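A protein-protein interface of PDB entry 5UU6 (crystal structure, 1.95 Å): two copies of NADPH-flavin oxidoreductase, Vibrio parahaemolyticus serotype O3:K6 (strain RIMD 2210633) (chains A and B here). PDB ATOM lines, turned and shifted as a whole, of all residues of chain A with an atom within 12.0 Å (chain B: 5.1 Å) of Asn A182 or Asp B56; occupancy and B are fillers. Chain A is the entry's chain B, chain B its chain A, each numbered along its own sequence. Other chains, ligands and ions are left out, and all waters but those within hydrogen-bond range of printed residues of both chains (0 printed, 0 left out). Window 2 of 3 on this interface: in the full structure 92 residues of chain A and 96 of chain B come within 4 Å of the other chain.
The backbone NH of Arg B53 sits at hydrogen-bond distance from the backbone carbonyl oxygen of His A180 (2.6 Å). The backbone NH (N) of Asn A182 is in hydrogen-bond range of the backbone carbonyl oxygen (O) of Arg B53 (2.7 Å). The backbone NH (N) of Thr B55 lies within hydrogen-bond range of the side-chain amide oxygen (OD1) of Asn A182 (2.9 Å). The backbone NH (N) of Asp B56 sits at hydrogen-bond distance from the side-chain amide oxygen (OD1) of Asn A182, 3.0 Å away. The side-chain amino group (NZ) of Lys B59 lies within hydrogen-bond range of the backbone carbonyl oxygen (O) of Asn A182, 2.6 Å away. The backbone carbonyl oxygen (O) of Leu B146 lies within hydrogen-bond range of the backbone NH (N) of Tyr A184, 3.0 Å away.
Of chain B, only Val B52 (3.7 Å), Arg B53 (2.7 Å), Val B54 (3.5 Å), Thr B55 (2.9 Å), Asp B56 (3.0 Å), Lys B59 (2.6 Å) and Leu B146 (3.8 Å) come within 4 Å of Asn A182. Asp B56 touches one residue of chain A. Printed residues of chain A within 4 Å of Val B54: Asn A182 (3.5 Å). No residue of chain A comes within 4 Å of Glu B58. No residue of chain A comes within 4 Å of Arg B60. Leu B145 touches none of the printed residues of chain A. Of the printed residues of chain A, Leu B146 touches Asn A182, Gln A183 and Tyr A184. Of the printed residues of chain B, Glu A181 touches Arg B53 (3.5 Å). Of the printed residues of chain B, Gln A183 touches Val B52, Lys B59 and Leu B146. The nearest residue of chain B that does not touch Asn A182 is Leu B145 (4.6 Å). The nearest residue of chain A that does not touch Asp B56 is Glu A181 (6.9 Å).
The backbone carbonyl oxygen (O) of Val B54 lies within hydrogen-bond range of the guanidinium group (NE) of Arg B60 (2.9 Å). N of Glu B58 sits at hydrogen-bond distance from OD2 of Asp B56 (3.3 Å). The backbone NH of Lys B59 lies within hydrogen-bond range of the side-chain carboxylate of Asp B56. O of Leu B145 sits at hydrogen-bond distance from NZ of Lys B59, at 2.8 Å. A ring nitrogen (ND1) of His A180 sits at hydrogen-bond distance from the backbone NH of Gln A185 (3.0 Å). O of Gln A183 lies within hydrogen-bond range of NE2 of Gln A185 (2.9 Å).
No position is printed for both chains. Of the 14 pairs that touch across the chains among the printed residues, none has its exchanged pair printed and touching as well.
Val B52 touches His A180. CA of Glu A181 touches O of Arg B53, 3.5 Å away. CG1 of Val B52 touches C of Asn A182 (3.7 Å). OD1 of Asn A182 touches CA of Val B54, at 3.5 Å. CD2 of Leu B146 touches O of Asn A182 (3.8 Å). CG1 of Val B52 touches N of Gln A183, 3.8 Å away. Gln A183 touches Lys B59. Leu B146 touches Gln A183 (O to CA, 3.3 Å).
Of the 12 printed residues of chain A, 5 touch a printed residue of chain B. Among the printed residues, 14 pairs touch across the chains.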
ATOM      1  N   ALA A 175      17.503   3.474  25.978  1.00  0.00           N
ATOM      2  CA  ALA A 175      16.672   4.669  25.895  1.00  0.00           C
ATOM      3  C   ALA A 175      16.498   5.135  24.458  1.00  0.00           C
ATOM      4  O   ALA A 175      15.462   5.711  24.132  1.00  0.00           O
ATOM      5  CB  ALA A 175      17.270   5.805  26.730  1.00  0.00           C
ATOM      6  N   HIS A 176      17.470   4.884  23.579  1.00  0.00           N
ATOM      7  CA  HIS A 176      17.262   5.311  22.195  1.00  0.00           C
ATOM      8  C   HIS A 176      16.304   4.394  21.438  1.00  0.00           C
ATOM      9  O   HIS A 176      15.916   4.715  20.313  1.00  0.00           O
ATOM     10  CB  HIS A 176      18.590   5.413  21.435  1.00  0.00           C
ATOM     11  CG  HIS A 176      19.163   4.092  21.016  1.00  0.00           C
ATOM     12  ND1 HIS A 176      20.154   3.453  21.731  1.00  0.00           N
ATOM     13  CD2 HIS A 176      18.916   3.310  19.936  1.00  0.00           C
ATOM     14  CE1 HIS A 176      20.476   2.322  21.125  1.00  0.00           C
ATOM     15  NE2 HIS A 176      19.742   2.212  20.031  1.00  0.00           N
ATOM     16  N   VAL A 177      15.928   3.261  22.011  1.00  0.00           N
ATOM     17  CA  VAL A 177      14.827   2.482  21.457  1.00  0.00           C
ATOM     18  C   VAL A 177      13.504   2.940  22.042  1.00  0.00           C
ATOM     19  O   VAL A 177      12.518   3.128  21.323  1.00  0.00           O
ATOM     20  CB  VAL A 177      15.070   0.976  21.705  1.00  0.00           C
ATOM     21  CG1 VAL A 177      13.794   0.142  21.432  1.00  0.00           C
ATOM     22  CG2 VAL A 177      16.235   0.505  20.856  1.00  0.00           C
ATOM     23  N   VAL A 178      13.475   3.164  23.344  1.00  0.00           N
ATOM     24  CA  VAL A 178      12.218   3.393  24.034  1.00  0.00           C
ATOM     25  C   VAL A 178      11.788   4.860  23.976  1.00  0.00           C
ATOM     26  O   VAL A 178      10.587   5.161  24.046  1.00  0.00           O
ATOM     27  CB  VAL A 178      12.366   2.892  25.485  1.00  0.00           C
ATOM     28  CG1 VAL A 178      11.173   3.250  26.307  1.00  0.00           C
ATOM     29  CG2 VAL A 178      12.558   1.377  25.482  1.00  0.00           C
ATOM     30  N   VAL A 179      12.740   5.775  23.840  1.00  0.00           N
ATOM     31  CA  VAL A 179      12.470   7.203  23.897  1.00  0.00           C
ATOM     32  C   VAL A 179      12.569   7.758  22.483  1.00  0.00           C
ATOM     33  O   VAL A 179      13.592   7.586  21.819  1.00  0.00           O
ATOM     34  CB  VAL A 179      13.435   7.926  24.847  1.00  0.00           C
ATOM     35  CG1 VAL A 179      13.032   9.402  24.956  1.00  0.00           C
ATOM     36  CG2 VAL A 179      13.437   7.199  26.227  1.00  0.00           C
ATOM     37  N   HIS A 180      11.498   8.394  22.023  1.00  0.00           N
ATOM     38  CA  HIS A 180      11.404   8.983  20.687  1.00  0.00           C
ATOM     39  C   HIS A 180      11.431  10.500  20.791  1.00  0.00           C
ATOM     40  O   HIS A 180      10.827  11.084  21.704  1.00  0.00           O
ATOM     41  CB  HIS A 180      10.107   8.581  19.984  1.00  0.00           C
ATOM     42  CG  HIS A 180       9.837   7.125  20.043  1.00  0.00           C
ATOM     43  ND1 HIS A 180      10.058   6.294  18.975  1.00  0.00           N
ATOM     44  CD2 HIS A 180       9.379   6.340  21.049  1.00  0.00           C
ATOM     45  CE1 HIS A 180       9.755   5.052  19.319  1.00  0.00           C
ATOM     46  NE2 HIS A 180       9.350   5.052  20.574  1.00  0.00           N
ATOM     47  N   GLU A 181      12.093  11.132  19.844  1.00  0.00           N
ATOM     48  CA  GLU A 181      12.179  12.589  19.799  1.00  0.00           C
ATOM     49  C   GLU A 181      11.161  13.127  18.797  1.00  0.00           C
ATOM     50  O   GLU A 181      11.248  12.849  17.599  1.00  0.00           O
ATOM     51  CB  GLU A 181      13.589  13.042  19.444  1.00  0.00           C
ATOM     52  CG  GLU A 181      13.960  14.321  20.164  1.00  0.00           C
ATOM     53  N   ASN A 182      10.171  13.853  19.315  1.00  0.00           N
ATOM     54  CA  ASN A 182       9.153  14.568  18.544  1.00  0.00           C
ATOM     55  C   ASN A 182       8.142  13.711  17.791  1.00  0.00           C
ATOM     56  O   ASN A 182       6.995  14.124  17.657  1.00  0.00           O
ATOM     57  CB  ASN A 182       9.818  15.537  17.573  1.00  0.00           C
ATOM     58  CG  ASN A 182      10.417  16.707  18.295  1.00  0.00           C
ATOM     59  OD1 ASN A 182       9.831  17.228  19.273  1.00  0.00           O
ATOM     60  ND2 ASN A 182      11.583  17.113  17.865  1.00  0.00           N
ATOM     61  N   GLN A 183       8.516  12.548  17.321  1.00  0.00           N
ATOM     62  CA  GLN A 183       7.586  11.662  16.653  1.00  0.00           C
ATOM     63  C   GLN A 183       8.004  10.223  16.744  1.00  0.00           C
ATOM     64  O   GLN A 183       9.129   9.936  16.846  1.00  0.00           O
ATOM     65  CB  GLN A 183       7.299  12.072  15.220  1.00  0.00           C
ATOM     66  CG  GLN A 183       8.536  12.090  14.376  1.00  0.00           C
ATOM     67  N   TYR A 184       7.054   9.336  16.680  1.00  0.00           N
ATOM     68  CA  TYR A 184       7.347   7.914  16.807  1.00  0.00           C
ATOM     69  C   TYR A 184       8.314   7.468  15.707  1.00  0.00           C
ATOM     70  O   TYR A 184       8.128   7.794  14.531  1.00  0.00           O
ATOM     71  CB  TYR A 184       6.051   7.097  16.741  1.00  0.00           C
ATOM     72  CG  TYR A 184       6.223   5.652  17.211  1.00  0.00           C
ATOM     73  CD1 TYR A 184       6.635   4.651  16.328  1.00  0.00           C
ATOM     74  CD2 TYR A 184       5.983   5.298  18.535  1.00  0.00           C
ATOM     75  CE1 TYR A 184       6.791   3.324  16.759  1.00  0.00           C
ATOM     76  CE2 TYR A 184       6.143   3.959  18.999  1.00  0.00           C
ATOM     77  CZ  TYR A 184       6.541   2.991  18.098  1.00  0.00           C
ATOM     78  OH  TYR A 184       6.682   1.684  18.528  1.00  0.00           O
ATOM     79  N   GLN A 185       9.360   6.742  16.109  1.00  0.00           N
ATOM     80  CA  GLN A 185      10.362   6.170  15.210  1.00  0.00           C
ATOM     81  C   GLN A 185      10.076   4.687  14.984  1.00  0.00           C
ATOM     82  O   GLN A 185       9.843   3.940  15.941  1.00  0.00           O
ATOM     83  CB  GLN A 185      11.769   6.337  15.800  1.00  0.00           C
ATOM     84  CG  GLN A 185      12.032   7.726  16.352  1.00  0.00           C
ATOM     85  CD  GLN A 185      12.222   8.743  15.242  1.00  0.00           C
ATOM     86  OE1 GLN A 185      12.926   8.473  14.270  1.00  0.00           O
ATOM     87  NE2 GLN A 185      11.577   9.908  15.370  1.00  0.00           N
ATOM     88  N   ASP A 186      10.099   4.274  13.725  1.00  0.00           N
ATOM     89  CA  ASP A 186       9.921   2.870  13.375  1.00  0.00           C
ATOM     90  C   ASP A 186      11.037   2.031  13.990  1.00  0.00           C
ATOM     91  O   ASP A 186      12.178   2.474  14.110  1.00  0.00           O
ATOM     92  CB  ASP A 186       9.928   2.699  11.859  1.00  0.00           C
ATOM     93  CG  ASP A 186       8.711   3.319  11.182  1.00  0.00           C
ATOM     94  OD1 ASP A 186       7.750   3.699  11.891  1.00  0.00           O
ATOM     95  OD2 ASP A 186       8.728   3.426   9.927  1.00  0.00           O
ATOM     96  N   VAL B  52       7.549   9.755  24.070  1.00  0.00           N
ATOM     97  CA  VAL B  52       7.928  10.737  23.059  1.00  0.00           C
ATOM     98  C   VAL B  52       8.357  12.010  23.776  1.00  0.00           C
ATOM     99  O   VAL B  52       7.572  12.642  24.495  1.00  0.00           O
ATOM    100  CB  VAL B  52       6.809  11.008  22.041  1.00  0.00           C
ATOM    101  CG1 VAL B  52       7.328  11.948  20.920  1.00  0.00           C
ATOM    102  CG2 VAL B  52       6.330   9.727  21.428  1.00  0.00           C
ATOM    103  N   ARG B  53       9.608  12.383  23.581  1.00  0.00           N
ATOM    104  CA  ARG B  53      10.143  13.619  24.123  1.00  0.00           C
ATOM    105  C   ARG B  53       9.893  14.718  23.086  1.00  0.00           C
ATOM    106  O   ARG B  53      10.264  14.560  21.919  1.00  0.00           O
ATOM    107  CB  ARG B  53      11.635  13.451  24.396  1.00  0.00           C
ATOM    108  CG  ARG B  53      12.276  14.632  25.038  1.00  0.00           C
ATOM    109  CD  ARG B  53      13.760  14.531  24.924  1.00  0.00           C
ATOM    110  NE  ARG B  53      14.311  15.829  25.220  1.00  0.00           N
ATOM    111  CZ  ARG B  53      15.462  16.298  24.779  1.00  0.00           C
ATOM    112  NH1 ARG B  53      16.244  15.550  23.990  1.00  0.00           N
ATOM    113  NH2 ARG B  53      15.834  17.518  25.171  1.00  0.00           N
ATOM    114  N   VAL B  54       9.237  15.809  23.491  1.00  0.00           N
ATOM    115  CA  VAL B  54       8.794  16.824  22.540  1.00  0.00           C
ATOM    116  C   VAL B  54       9.620  18.077  22.769  1.00  0.00           C
ATOM    117  O   VAL B  54       9.451  18.774  23.775  1.00  0.00           O
ATOM    118  CB  VAL B  54       7.293  17.119  22.655  1.00  0.00           C
ATOM    119  CG1 VAL B  54       6.881  18.181  21.607  1.00  0.00           C
ATOM    120  CG2 VAL B  54       6.460  15.815  22.474  1.00  0.00           C
ATOM    121  N   THR B  55      10.522  18.346  21.831  1.00  0.00           N
ATOM    122  CA  THR B  55      11.384  19.512  21.854  1.00  0.00           C
ATOM    123  C   THR B  55      10.993  20.565  20.830  1.00  0.00           C
ATOM    124  O   THR B  55      11.351  21.736  21.003  1.00  0.00           O
ATOM    125  CB  THR B  55      12.841  19.103  21.596  1.00  0.00           C
ATOM    126  OG1 THR B  55      12.912  18.429  20.332  1.00  0.00           O
ATOM    127  CG2 THR B  55      13.347  18.178  22.707  1.00  0.00           C
ATOM    128  N   ASP B  56      10.280  20.179  19.777  1.00  0.00           N
ATOM    129  CA  ASP B  56       9.840  21.145  18.783  1.00  0.00           C
ATOM    130  C   ASP B  56       8.804  22.091  19.390  1.00  0.00           C
ATOM    131  O   ASP B  56       7.758  21.653  19.896  1.00  0.00           O
ATOM    132  CB  ASP B  56       9.265  20.435  17.570  1.00  0.00           C
ATOM    133  CG  ASP B  56       8.674  21.419  16.560  1.00  0.00           C
ATOM    134  OD1 ASP B  56       9.443  22.116  15.859  1.00  0.00           O
ATOM    135  OD2 ASP B  56       7.438  21.514  16.485  1.00  0.00           O
ATOM    136  N   ILE B  57       9.072  23.397  19.295  1.00  0.00           N
ATOM    137  CA  ILE B  57       8.250  24.367  20.014  1.00  0.00           C
ATOM    138  C   ILE B  57       6.849  24.505  19.396  1.00  0.00           C
ATOM    139  O   ILE B  57       5.881  24.789  20.111  1.00  0.00           O
ATOM    140  CB  ILE B  57       8.985  25.719  20.108  1.00  0.00           C
ATOM    141  CG1 ILE B  57       9.260  26.299  18.735  1.00  0.00           C
ATOM    142  CG2 ILE B  57      10.344  25.566  20.821  1.00  0.00           C
ATOM    143  CD1 ILE B  57      10.188  27.525  18.805  1.00  0.00           C
ATOM    144  N   GLU B  58       6.702  24.326  18.082  1.00  0.00           N
ATOM    145  CA  GLU B  58       5.351  24.356  17.509  1.00  0.00           C
ATOM    146  C   GLU B  58       4.499  23.186  18.009  1.00  0.00           C
ATOM    147  O   GLU B  58       3.304  23.354  18.285  1.00  0.00           O
ATOM    148  CB  GLU B  58       5.415  24.354  15.983  1.00  0.00           C
ATOM    149  N   LYS B  59       5.078  21.981  18.100  1.00  0.00           N
ATOM    150  CA  LYS B  59       4.330  20.859  18.672  1.00  0.00           C
ATOM    151  C   LYS B  59       4.034  21.096  20.144  1.00  0.00           C
ATOM    152  O   LYS B  59       2.961  20.744  20.633  1.00  0.00           O
ATOM    153  CB  LYS B  59       5.089  19.544  18.492  1.00  0.00           C
ATOM    154  CG  LYS B  59       5.251  19.092  17.055  1.00  0.00           C
ATOM    155  CD  LYS B  59       5.849  17.697  17.052  1.00  0.00           C
ATOM    156  CE  LYS B  59       5.600  16.970  15.763  1.00  0.00           C
ATOM    157  NZ  LYS B  59       5.550  15.511  16.000  1.00  0.00           N
ATOM    158  N   ARG B  60       4.987  21.666  20.872  1.00  0.00           N
ATOM    159  CA  ARG B  60       4.729  22.047  22.251  1.00  0.00           C
ATOM    160  C   ARG B  60       3.519  22.970  22.345  1.00  0.00           C
ATOM    161  O   ARG B  60       2.636  22.768  23.185  1.00  0.00           O
ATOM    162  CB  ARG B  60       5.990  22.709  22.835  1.00  0.00           C
ATOM    163  CG  ARG B  60       6.131  22.504  24.322  1.00  0.00           C
ATOM    164  CD  ARG B  60       6.398  21.035  24.741  1.00  0.00           C
ATOM    165  NE  ARG B  60       7.831  20.824  25.022  1.00  0.00           N
ATOM    166  CZ  ARG B  60       8.497  21.421  26.012  1.00  0.00           C
ATOM    167  NH1 ARG B  60       7.872  22.244  26.857  1.00  0.00           N
ATOM    168  NH2 ARG B  60       9.791  21.172  26.174  1.00  0.00           N
ATOM    169  N   LEU B 145      -0.577  14.002  15.902  1.00  0.00           N
ATOM    170  CA  LEU B 145       0.517  14.963  15.946  1.00  0.00           C
ATOM    171  C   LEU B 145       1.858  14.278  16.223  1.00  0.00           C
ATOM    172  O   LEU B 145       2.888  14.699  15.697  1.00  0.00           O
ATOM    173  CB  LEU B 145       0.205  16.028  17.012  1.00  0.00           C
ATOM    174  CG  LEU B 145       1.282  17.090  17.263  1.00  0.00           C
ATOM    175  CD1 LEU B 145       1.370  18.162  16.106  1.00  0.00           C
ATOM    176  CD2 LEU B 145       1.176  17.739  18.617  1.00  0.00           C
ATOM    177  N   LEU B 146       1.868  13.209  17.023  1.00  0.00           N
ATOM    178  CA  LEU B 146       3.113  12.529  17.365  1.00  0.00           C
ATOM    179  C   LEU B 146       3.424  11.372  16.430  1.00  0.00           C
ATOM    180  O   LEU B 146       4.409  10.664  16.665  1.00  0.00           O
ATOM    181  CB  LEU B 146       3.074  12.013  18.806  1.00  0.00           C
ATOM    182  CG  LEU B 146       2.839  13.081  19.879  1.00  0.00           C
ATOM    183  CD1 LEU B 146       2.774  12.462  21.266  1.00  0.00           C
ATOM    184  CD2 LEU B 146       3.879  14.190  19.850  1.00  0.00           C
